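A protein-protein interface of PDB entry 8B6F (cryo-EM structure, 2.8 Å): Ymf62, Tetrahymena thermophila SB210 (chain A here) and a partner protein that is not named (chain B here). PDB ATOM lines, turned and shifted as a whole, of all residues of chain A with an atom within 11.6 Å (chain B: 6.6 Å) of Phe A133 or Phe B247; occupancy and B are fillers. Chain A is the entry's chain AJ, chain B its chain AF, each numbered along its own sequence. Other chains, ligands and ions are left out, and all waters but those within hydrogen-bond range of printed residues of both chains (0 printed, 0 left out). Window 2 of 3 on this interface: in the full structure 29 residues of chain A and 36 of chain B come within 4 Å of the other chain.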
ATOM      1  N   LEU A  43       4.646  -7.800  19.779  1.00  0.00           N
ATOM      2  CA  LEU A  43       4.271  -6.654  20.600  1.00  0.00           C
ATOM      3  C   LEU A  43       5.493  -6.014  21.245  1.00  0.00           C
ATOM      4  O   LEU A  43       5.546  -4.790  21.409  1.00  0.00           O
ATOM      5  CB  LEU A  43       3.255  -7.076  21.659  1.00  0.00           C
ATOM      6  CG  LEU A  43       1.938  -7.635  21.119  1.00  0.00           C
ATOM      7  CD1 LEU A  43       1.072  -8.131  22.255  1.00  0.00           C
ATOM      8  CD2 LEU A  43       1.195  -6.594  20.301  1.00  0.00           C
ATOM      9  N   PRO A 124      -3.990   7.113  27.505  1.00  0.00           N
ATOM     10  CA  PRO A 124      -5.448   7.028  27.683  1.00  0.00           C
ATOM     11  C   PRO A 124      -6.190   6.720  26.397  1.00  0.00           C
ATOM     12  O   PRO A 124      -7.158   5.950  26.415  1.00  0.00           O
ATOM     13  CB  PRO A 124      -5.821   8.413  28.234  1.00  0.00           C
ATOM     14  CG  PRO A 124      -4.535   9.077  28.585  1.00  0.00           C
ATOM     15  CD  PRO A 124      -3.506   8.490  27.689  1.00  0.00           C
ATOM     16  N   SER A 125      -5.758   7.298  25.275  1.00  0.00           N
ATOM     17  CA  SER A 125      -6.406   7.010  24.001  1.00  0.00           C
ATOM     18  C   SER A 125      -6.267   5.538  23.638  1.00  0.00           C
ATOM     19  O   SER A 125      -7.224   4.915  23.163  1.00  0.00           O
ATOM     20  CB  SER A 125      -5.822   7.894  22.900  1.00  0.00           C
ATOM     21  OG  SER A 125      -4.447   7.623  22.704  1.00  0.00           O
ATOM     22  N   LEU A 126      -5.081   4.965  23.847  1.00  0.00           N
ATOM     23  CA  LEU A 126      -4.906   3.538  23.601  1.00  0.00           C
ATOM     24  C   LEU A 126      -5.780   2.708  24.530  1.00  0.00           C
ATOM     25  O   LEU A 126      -6.344   1.689  24.115  1.00  0.00           O
ATOM     26  CB  LEU A 126      -3.441   3.143  23.768  1.00  0.00           C
ATOM     27  CG  LEU A 126      -3.188   1.634  23.681  1.00  0.00           C
ATOM     28  CD1 LEU A 126      -3.646   1.079  22.346  1.00  0.00           C
ATOM     29  CD2 LEU A 126      -1.735   1.335  23.884  1.00  0.00           C
ATOM     30  N   VAL A 127      -5.903   3.119  25.792  1.00  0.00           N
ATOM     31  CA  VAL A 127      -6.743   2.377  26.727  1.00  0.00           C
ATOM     32  C   VAL A 127      -8.183   2.358  26.231  1.00  0.00           C
ATOM     33  O   VAL A 127      -8.837   1.308  26.209  1.00  0.00           O
ATOM     34  CB  VAL A 127      -6.632   2.976  28.141  1.00  0.00           C
ATOM     35  CG1 VAL A 127      -7.771   2.495  29.027  1.00  0.00           C
ATOM     36  CG2 VAL A 127      -5.293   2.616  28.765  1.00  0.00           C
ATOM     37  N   LEU A 128      -8.701   3.518  25.825  1.00  0.00           N
ATOM     38  CA  LEU A 128     -10.071   3.572  25.328  1.00  0.00           C
ATOM     39  C   LEU A 128     -10.234   2.726  24.074  1.00  0.00           C
ATOM     40  O   LEU A 128     -11.218   1.991  23.934  1.00  0.00           O
ATOM     41  CB  LEU A 128     -10.478   5.019  25.050  1.00  0.00           C
ATOM     42  CG  LEU A 128     -10.628   5.936  26.263  1.00  0.00           C
ATOM     43  CD1 LEU A 128     -10.940   7.348  25.809  1.00  0.00           C
ATOM     44  CD2 LEU A 128     -11.707   5.431  27.209  1.00  0.00           C
ATOM     45  N   PHE A 129      -9.283   2.822  23.143  1.00  0.00           N
ATOM     46  CA  PHE A 129      -9.388   2.057  21.907  1.00  0.00           C
ATOM     47  C   PHE A 129      -9.375   0.560  22.184  1.00  0.00           C
ATOM     48  O   PHE A 129     -10.172  -0.190  21.612  1.00  0.00           O
ATOM     49  CB  PHE A 129      -8.251   2.435  20.960  1.00  0.00           C
ATOM     50  CG  PHE A 129      -8.301   1.718  19.645  1.00  0.00           C
ATOM     51  CD1 PHE A 129      -9.142   2.156  18.637  1.00  0.00           C
ATOM     52  CD2 PHE A 129      -7.506   0.608  19.417  1.00  0.00           C
ATOM     53  CE1 PHE A 129      -9.192   1.500  17.424  1.00  0.00           C
ATOM     54  CE2 PHE A 129      -7.551  -0.054  18.206  1.00  0.00           C
ATOM     55  CZ  PHE A 129      -8.396   0.394  17.207  1.00  0.00           C
ATOM     56  N   LEU A 130      -8.490   0.108  23.075  1.00  0.00           N
ATOM     57  CA  LEU A 130      -8.449  -1.311  23.417  1.00  0.00           C
ATOM     58  C   LEU A 130      -9.733  -1.752  24.105  1.00  0.00           C
ATOM     59  O   LEU A 130     -10.231  -2.856  23.855  1.00  0.00           O
ATOM     60  CB  LEU A 130      -7.242  -1.607  24.306  1.00  0.00           C
ATOM     61  CG  LEU A 130      -5.861  -1.458  23.664  1.00  0.00           C
ATOM     62  CD1 LEU A 130      -4.780  -1.769  24.680  1.00  0.00           C
ATOM     63  CD2 LEU A 130      -5.717  -2.356  22.446  1.00  0.00           C
ATOM     64  N   ILE A 131     -10.285  -0.906  24.973  1.00  0.00           N
ATOM     65  CA  ILE A 131     -11.521  -1.263  25.660  1.00  0.00           C
ATOM     66  C   ILE A 131     -12.650  -1.471  24.658  1.00  0.00           C
ATOM     67  O   ILE A 131     -13.422  -2.431  24.767  1.00  0.00           O
ATOM     68  CB  ILE A 131     -11.879  -0.183  26.702  1.00  0.00           C
ATOM     69  CG1 ILE A 131     -10.901  -0.221  27.883  1.00  0.00           C
ATOM     70  CG2 ILE A 131     -13.327  -0.329  27.176  1.00  0.00           C
ATOM     71  CD1 ILE A 131     -11.122  -1.367  28.851  1.00  0.00           C
ATOM     72  N   PHE A 132     -12.773  -0.579  23.678  1.00  0.00           N
ATOM     73  CA  PHE A 132     -13.940  -0.553  22.807  1.00  0.00           C
ATOM     74  C   PHE A 132     -13.695  -1.143  21.423  1.00  0.00           C
ATOM     75  O   PHE A 132     -14.577  -1.044  20.566  1.00  0.00           O
ATOM     76  CB  PHE A 132     -14.442   0.881  22.665  1.00  0.00           C
ATOM     77  CG  PHE A 132     -15.016   1.430  23.925  1.00  0.00           C
ATOM     78  CD1 PHE A 132     -16.192   0.923  24.433  1.00  0.00           C
ATOM     79  CD2 PHE A 132     -14.382   2.457  24.604  1.00  0.00           C
ATOM     80  CE1 PHE A 132     -16.721   1.415  25.593  1.00  0.00           C
ATOM     81  CE2 PHE A 132     -14.910   2.960  25.772  1.00  0.00           C
ATOM     82  CZ  PHE A 132     -16.086   2.440  26.267  1.00  0.00           C
ATOM     83  N   PHE A 133     -12.544  -1.765  21.180  1.00  0.00           N
ATOM     84  CA  PHE A 133     -12.210  -2.269  19.854  1.00  0.00           C
ATOM     85  C   PHE A 133     -12.072  -3.782  19.897  1.00  0.00           C
ATOM     86  O   PHE A 133     -11.177  -4.311  20.565  1.00  0.00           O
ATOM     87  CB  PHE A 133     -10.919  -1.640  19.330  1.00  0.00           C
ATOM     88  CG  PHE A 133     -10.511  -2.148  17.979  1.00  0.00           C
ATOM     89  CD1 PHE A 133     -11.086  -1.637  16.829  1.00  0.00           C
ATOM     90  CD2 PHE A 133      -9.557  -3.144  17.863  1.00  0.00           C
ATOM     91  CE1 PHE A 133     -10.713  -2.109  15.588  1.00  0.00           C
ATOM     92  CE2 PHE A 133      -9.180  -3.620  16.624  1.00  0.00           C
ATOM     93  CZ  PHE A 133      -9.759  -3.101  15.486  1.00  0.00           C
ATOM     94  N   ASN A 134     -12.954  -4.471  19.177  1.00  0.00           N
ATOM     95  CA  ASN A 134     -12.776  -5.891  18.892  1.00  0.00           C
ATOM     96  C   ASN A 134     -13.624  -6.212  17.672  1.00  0.00           C
ATOM     97  O   ASN A 134     -14.855  -6.156  17.746  1.00  0.00           O
ATOM     98  CB  ASN A 134     -13.171  -6.752  20.082  1.00  0.00           C
ATOM     99  CG  ASN A 134     -12.868  -8.219  19.860  1.00  0.00           C
ATOM    100  OD1 ASN A 134     -13.748  -9.001  19.503  1.00  0.00           O
ATOM    101  ND2 ASN A 134     -11.611  -8.600  20.061  1.00  0.00           N
ATOM    102  N   ILE A 135     -12.973  -6.540  16.557  1.00  0.00           N
ATOM    103  CA  ILE A 135     -13.704  -6.885  15.344  1.00  0.00           C
ATOM    104  C   ILE A 135     -13.908  -8.388  15.204  1.00  0.00           C
ATOM    105  O   ILE A 135     -14.839  -8.814  14.507  1.00  0.00           O
ATOM    106  CB  ILE A 135     -12.988  -6.342  14.096  1.00  0.00           C
ATOM    107  CG1 ILE A 135     -12.669  -4.854  14.263  1.00  0.00           C
ATOM    108  CG2 ILE A 135     -13.862  -6.545  12.871  1.00  0.00           C
ATOM    109  CD1 ILE A 135     -11.874  -4.257  13.115  1.00  0.00           C
ATOM    110  N   ASP A 136     -13.077  -9.202  15.846  1.00  0.00           N
ATOM    111  CA  ASP A 136     -13.261 -10.647  15.792  1.00  0.00           C
ATOM    112  C   ASP A 136     -14.619 -11.016  16.371  1.00  0.00           C
ATOM    113  O   ASP A 136     -14.879 -10.795  17.557  1.00  0.00           O
ATOM    114  CB  ASP A 136     -12.137 -11.339  16.558  1.00  0.00           C
ATOM    115  CG  ASP A 136     -12.183 -12.842  16.427  1.00  0.00           C
ATOM    116  OD1 ASP A 136     -12.211 -13.336  15.282  1.00  0.00           O
ATOM    117  OD2 ASP A 136     -12.181 -13.533  17.465  1.00  0.00           O
ATOM    118  N   TYR A 137     -15.483 -11.584  15.529  1.00  0.00           N
ATOM    119  CA  TYR A 137     -16.864 -11.834  15.929  1.00  0.00           C
ATOM    120  C   TYR A 137     -16.981 -13.101  16.770  1.00  0.00           C
ATOM    121  O   TYR A 137     -17.340 -13.043  17.951  1.00  0.00           O
ATOM    122  CB  TYR A 137     -17.749 -11.930  14.679  1.00  0.00           C
ATOM    123  CG  TYR A 137     -19.244 -11.898  14.939  1.00  0.00           C
ATOM    124  CD1 TYR A 137     -19.755 -11.801  16.228  1.00  0.00           C
ATOM    125  CD2 TYR A 137     -20.144 -11.972  13.885  1.00  0.00           C
ATOM    126  CE1 TYR A 137     -21.117 -11.775  16.457  1.00  0.00           C
ATOM    127  CE2 TYR A 137     -21.507 -11.947  14.105  1.00  0.00           C
ATOM    128  CZ  TYR A 137     -21.987 -11.849  15.393  1.00  0.00           C
ATOM    129  OH  TYR A 137     -23.343 -11.824  15.617  1.00  0.00           O
ATOM    130  N   PHE B 209      -7.744  -1.967   3.991  1.00  0.00           N
ATOM    131  CA  PHE B 209      -8.324  -2.632   5.151  1.00  0.00           C
ATOM    132  C   PHE B 209      -9.824  -2.816   4.970  1.00  0.00           C
ATOM    133  O   PHE B 209     -10.370  -3.881   5.277  1.00  0.00           O
ATOM    134  CB  PHE B 209      -8.021  -1.827   6.415  1.00  0.00           C
ATOM    135  CG  PHE B 209      -8.556  -2.445   7.674  1.00  0.00           C
ATOM    136  CD1 PHE B 209      -9.828  -2.137   8.126  1.00  0.00           C
ATOM    137  CD2 PHE B 209      -7.779  -3.316   8.415  1.00  0.00           C
ATOM    138  CE1 PHE B 209     -10.319  -2.698   9.286  1.00  0.00           C
ATOM    139  CE2 PHE B 209      -8.265  -3.881   9.576  1.00  0.00           C
ATOM    140  CZ  PHE B 209      -9.537  -3.572  10.012  1.00  0.00           C
ATOM    141  N   TYR B 213     -11.950  -6.416   4.778  1.00  0.00           N
ATOM    142  CA  TYR B 213     -13.058  -6.765   5.658  1.00  0.00           C
ATOM    143  C   TYR B 213     -14.374  -6.886   4.902  1.00  0.00           C
ATOM    144  O   TYR B 213     -15.257  -7.641   5.323  1.00  0.00           O
ATOM    145  CB  TYR B 213     -13.174  -5.752   6.792  1.00  0.00           C
ATOM    146  CG  TYR B 213     -12.628  -6.312   8.075  1.00  0.00           C
ATOM    147  CD1 TYR B 213     -13.383  -7.182   8.848  1.00  0.00           C
ATOM    148  CD2 TYR B 213     -11.346  -6.001   8.498  1.00  0.00           C
ATOM    149  CE1 TYR B 213     -12.881  -7.715  10.012  1.00  0.00           C
ATOM    150  CE2 TYR B 213     -10.835  -6.528   9.660  1.00  0.00           C
ATOM    151  CZ  TYR B 213     -11.607  -7.381  10.414  1.00  0.00           C
ATOM    152  OH  TYR B 213     -11.093  -7.901  11.573  1.00  0.00           O
ATOM    153  N   ASN B 242     -22.683  -5.377  14.874  1.00  0.00           N
ATOM    154  CA  ASN B 242     -22.777  -3.941  14.649  1.00  0.00           C
ATOM    155  C   ASN B 242     -21.422  -3.266  14.796  1.00  0.00           C
ATOM    156  O   ASN B 242     -21.143  -2.279  14.108  1.00  0.00           O
ATOM    157  CB  ASN B 242     -23.783  -3.324  15.620  1.00  0.00           C
ATOM    158  CG  ASN B 242     -25.171  -3.912  15.471  1.00  0.00           C
ATOM    159  OD1 ASN B 242     -25.566  -4.334  14.384  1.00  0.00           O
ATOM    160  ND2 ASN B 242     -25.918  -3.945  16.565  1.00  0.00           N
ATOM    161  N   ILE B 243     -20.573  -3.772  15.690  1.00  0.00           N
ATOM    162  CA  ILE B 243     -19.242  -3.199  15.852  1.00  0.00           C
ATOM    163  C   ILE B 243     -18.459  -3.310  14.549  1.00  0.00           C
ATOM    164  O   ILE B 243     -17.855  -2.338  14.084  1.00  0.00           O
ATOM    165  CB  ILE B 243     -18.501  -3.889  17.012  1.00  0.00           C
ATOM    166  CG1 ILE B 243     -19.287  -3.728  18.316  1.00  0.00           C
ATOM    167  CG2 ILE B 243     -17.097  -3.311  17.163  1.00  0.00           C
ATOM    168  CD1 ILE B 243     -18.693  -4.477  19.494  1.00  0.00           C
ATOM    169  N   THR B 244     -18.455  -4.500  13.943  1.00  0.00           N
ATOM    170  CA  THR B 244     -17.703  -4.688  12.706  1.00  0.00           C
ATOM    171  C   THR B 244     -18.274  -3.848  11.570  1.00  0.00           C
ATOM    172  O   THR B 244     -17.521  -3.216  10.822  1.00  0.00           O
ATOM    173  CB  THR B 244     -17.694  -6.167  12.320  1.00  0.00           C
ATOM    174  OG1 THR B 244     -17.107  -6.936  13.375  1.00  0.00           O
ATOM    175  CG2 THR B 244     -16.906  -6.389  11.034  1.00  0.00           C
ATOM    176  N   LEU B 245     -19.601  -3.825  11.424  1.00  0.00           N
ATOM    177  CA  LEU B 245     -20.205  -3.037  10.356  1.00  0.00           C
ATOM    178  C   LEU B 245     -19.897  -1.559  10.540  1.00  0.00           C
ATOM    179  O   LEU B 245     -19.538  -0.862   9.586  1.00  0.00           O
ATOM    180  CB  LEU B 245     -21.714  -3.273  10.313  1.00  0.00           C
ATOM    181  CG  LEU B 245     -22.157  -4.679   9.901  1.00  0.00           C
ATOM    182  CD1 LEU B 245     -23.652  -4.841  10.102  1.00  0.00           C
ATOM    183  CD2 LEU B 245     -21.782  -4.965   8.458  1.00  0.00           C
ATOM    184  N   LEU B 246     -20.044  -1.063  11.767  1.00  0.00           N
ATOM    185  CA  LEU B 246     -19.750   0.339  12.036  1.00  0.00           C
ATOM    186  C   LEU B 246     -18.285   0.658  11.774  1.00  0.00           C
ATOM    187  O   LEU B 246     -17.959   1.726  11.245  1.00  0.00           O
ATOM    188  CB  LEU B 246     -20.122   0.673  13.480  1.00  0.00           C
ATOM    189  CG  LEU B 246     -19.679   2.038  14.005  1.00  0.00           C
ATOM    190  CD1 LEU B 246     -20.291   3.161  13.185  1.00  0.00           C
ATOM    191  CD2 LEU B 246     -20.051   2.162  15.470  1.00  0.00           C
ATOM    192  N   PHE B 247     -17.384  -0.256  12.137  1.00  0.00           N
ATOM    193  CA  PHE B 247     -15.962  -0.002  11.936  1.00  0.00           C
ATOM    194  C   PHE B 247     -15.594  -0.011  10.458  1.00  0.00           C
ATOM    195  O   PHE B 247     -14.752   0.781  10.021  1.00  0.00           O
ATOM    196  CB  PHE B 247     -15.123  -1.023  12.698  1.00  0.00           C
ATOM    197  CG  PHE B 247     -13.689  -0.621  12.832  1.00  0.00           C
ATOM    198  CD1 PHE B 247     -13.310   0.306  13.789  1.00  0.00           C
ATOM    199  CD2 PHE B 247     -12.723  -1.143  11.990  1.00  0.00           C
ATOM    200  CE1 PHE B 247     -11.995   0.692  13.918  1.00  0.00           C
ATOM    201  CE2 PHE B 247     -11.403  -0.757  12.114  1.00  0.00           C
ATOM    202  CZ  PHE B 247     -11.040   0.162  13.080  1.00  0.00           C
ATOM    203  N   ILE B 248     -16.206  -0.897   9.672  1.00  0.00           N
ATOM    204  CA  ILE B 248     -15.966  -0.888   8.231  1.00  0.00           C
ATOM    205  C   ILE B 248     -16.417   0.439   7.637  1.00  0.00           C
ATOM    206  O   ILE B 248     -15.702   1.064   6.846  1.00  0.00           O
ATOM    207  CB  ILE B 248     -16.678  -2.081   7.564  1.00  0.00           C
ATOM    208  CG1 ILE B 248     -16.008  -3.392   7.979  1.00  0.00           C
ATOM    209  CG2 ILE B 248     -16.681  -1.938   6.044  1.00  0.00           C
ATOM    210  CD1 ILE B 248     -16.772  -4.635   7.568  1.00  0.00           C
ATOM    211  N   CYS B 249     -17.614   0.886   8.009  1.00  0.00           N
ATOM    212  CA  CYS B 249     -18.118   2.158   7.509  1.00  0.00           C
ATOM    213  C   CYS B 249     -17.210   3.306   7.927  1.00  0.00           C
ATOM    214  O   CYS B 249     -16.912   4.198   7.126  1.00  0.00           O
ATOM    215  CB  CYS B 249     -19.544   2.373   8.003  1.00  0.00           C
ATOM    216  SG  CYS B 249     -20.688   1.175   7.298  1.00  0.00           S
ATOM    217  N   LEU B 250     -16.768   3.306   9.184  1.00  0.00           N
ATOM    218  CA  LEU B 250     -15.893   4.367   9.663  1.00  0.00           C
ATOM    219  C   LEU B 250     -14.571   4.373   8.914  1.00  0.00           C
ATOM    220  O   LEU B 250     -14.069   5.435   8.532  1.00  0.00           O
ATOM    221  CB  LEU B 250     -15.638   4.185  11.154  1.00  0.00           C
ATOM    222  CG  LEU B 250     -16.819   4.544  12.040  1.00  0.00           C
ATOM    223  CD1 LEU B 250     -16.619   3.907  13.387  1.00  0.00           C
ATOM    224  CD2 LEU B 250     -16.935   6.054  12.159  1.00  0.00           C
ATOM    225  N   THR B 251     -13.992   3.195   8.694  1.00  0.00           N
ATOM    226  CA  THR B 251     -12.722   3.133   7.983  1.00  0.00           C
ATOM    227  C   THR B 251     -12.869   3.664   6.564  1.00  0.00           C
ATOM    228  O   THR B 251     -12.025   4.431   6.090  1.00  0.00           O
ATOM    229  CB  THR B 251     -12.198   1.697   7.972  1.00  0.00           C
ATOM    230  OG1 THR B 251     -12.057   1.227   9.317  1.00  0.00           O
ATOM    231  CG2 THR B 251     -10.848   1.622   7.278  1.00  0.00           C
ATOM    232  N   LEU B 252     -13.935   3.263   5.869  1.00  0.00           N
ATOM    233  CA  LEU B 252     -14.147   3.750   4.511  1.00  0.00           C
ATOM    234  C   LEU B 252     -14.330   5.263   4.492  1.00  0.00           C
ATOM    235  O   LEU B 252     -13.704   5.966   3.692  1.00  0.00           O
ATOM    236  CB  LEU B 252     -15.360   3.056   3.895  1.00  0.00           C
ATOM    237  CG  LEU B 252     -15.670   3.400   2.437  1.00  0.00           C
ATOM    238  CD1 LEU B 252     -14.454   3.192   1.546  1.00  0.00           C
ATOM    239  CD2 LEU B 252     -16.831   2.568   1.934  1.00  0.00           C
ATOM    240  N   PHE B 310     -25.854   2.968   8.803  1.00  0.00           N
ATOM    241  CA  PHE B 310     -24.674   3.368   9.559  1.00  0.00           C
ATOM    242  C   PHE B 310     -24.059   4.667   9.063  1.00  0.00           C
ATOM    243  O   PHE B 310     -23.522   5.432   9.869  1.00  0.00           O
ATOM    244  CB  PHE B 310     -23.606   2.271   9.498  1.00  0.00           C
ATOM    245  CG  PHE B 310     -23.994   0.994  10.187  1.00  0.00           C
ATOM    246  CD1 PHE B 310     -23.792   0.836  11.547  1.00  0.00           C
ATOM    247  CD2 PHE B 310     -24.534  -0.060   9.469  1.00  0.00           C
ATOM    248  CE1 PHE B 310     -24.139  -0.343  12.181  1.00  0.00           C
ATOM    249  CE2 PHE B 310     -24.884  -1.240  10.096  1.00  0.00           C
ATOM    250  CZ  PHE B 310     -24.685  -1.381  11.454  1.00  0.00           C
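The backbone carbonyl oxygen (O) of Ile A135 is in hydrogen-bond range of the side-chain hydroxyl (OG1) of Thr B244, 3.2 Å away.
The side-chain hydroxyl (OG1) of Thr B251 is in hydrogen-bond range of the backbone carbonyl oxygen (O) of Phe B247, 2.8 Å away. The backbone carbonyl oxygen (O) of Asp A136 lies close to the side-chain amide oxygen (OD1) of Asn A134.
Among the printed residues, merely in contact across the chains: Ile A135 with Tyr B213, Phe A133 with Phe B247, Ile A135 with Phe B247, Asn A134 with Ile B243 and Ile A135 with Phe B209.
Phe A133 touches just one residue of chain B: Phe B247 (3.4 Å). Of chain A, only Phe A133 and Ile A135 come within 4 Å of Phe B247. Thr B244 touches one residue of chain A. No residue of chain A comes within 4 Å of Ile B248. No residue of chain A comes within 4 Å of Cys B249. Printed residues of chain A within 4 Å of Phe B209: Ile A135. Printed residues of chain A within 4 Å of Tyr B213: Ile A135. Printed residues of chain B within 4 Å of Ile A135: Phe B209 (3.9 Å), Tyr B213 (3.2 Å), Thr B244 (3.2 Å) and Phe B247 (3.4 Å). Printed residues of chain B within 4 Å of Asn A134: Ile B243 (3.7 Å). Leu B252 touches none of the printed residues of chain A. Tyr A137 touches none of the printed residues of chain B. The nearest residue of chain B that does not touch Phe A133 is Phe B209 (5.5 Å). The nearest printed residue of chain A that does not touch Phe B209 is Phe A133 (5.5 Å).
Hydrophobic or aromatic side chains of chain A within 4 Å of the printed part of chain B: Phe A133 and Ile A135. Among the printed residues, 6 pairs touch across the chains.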
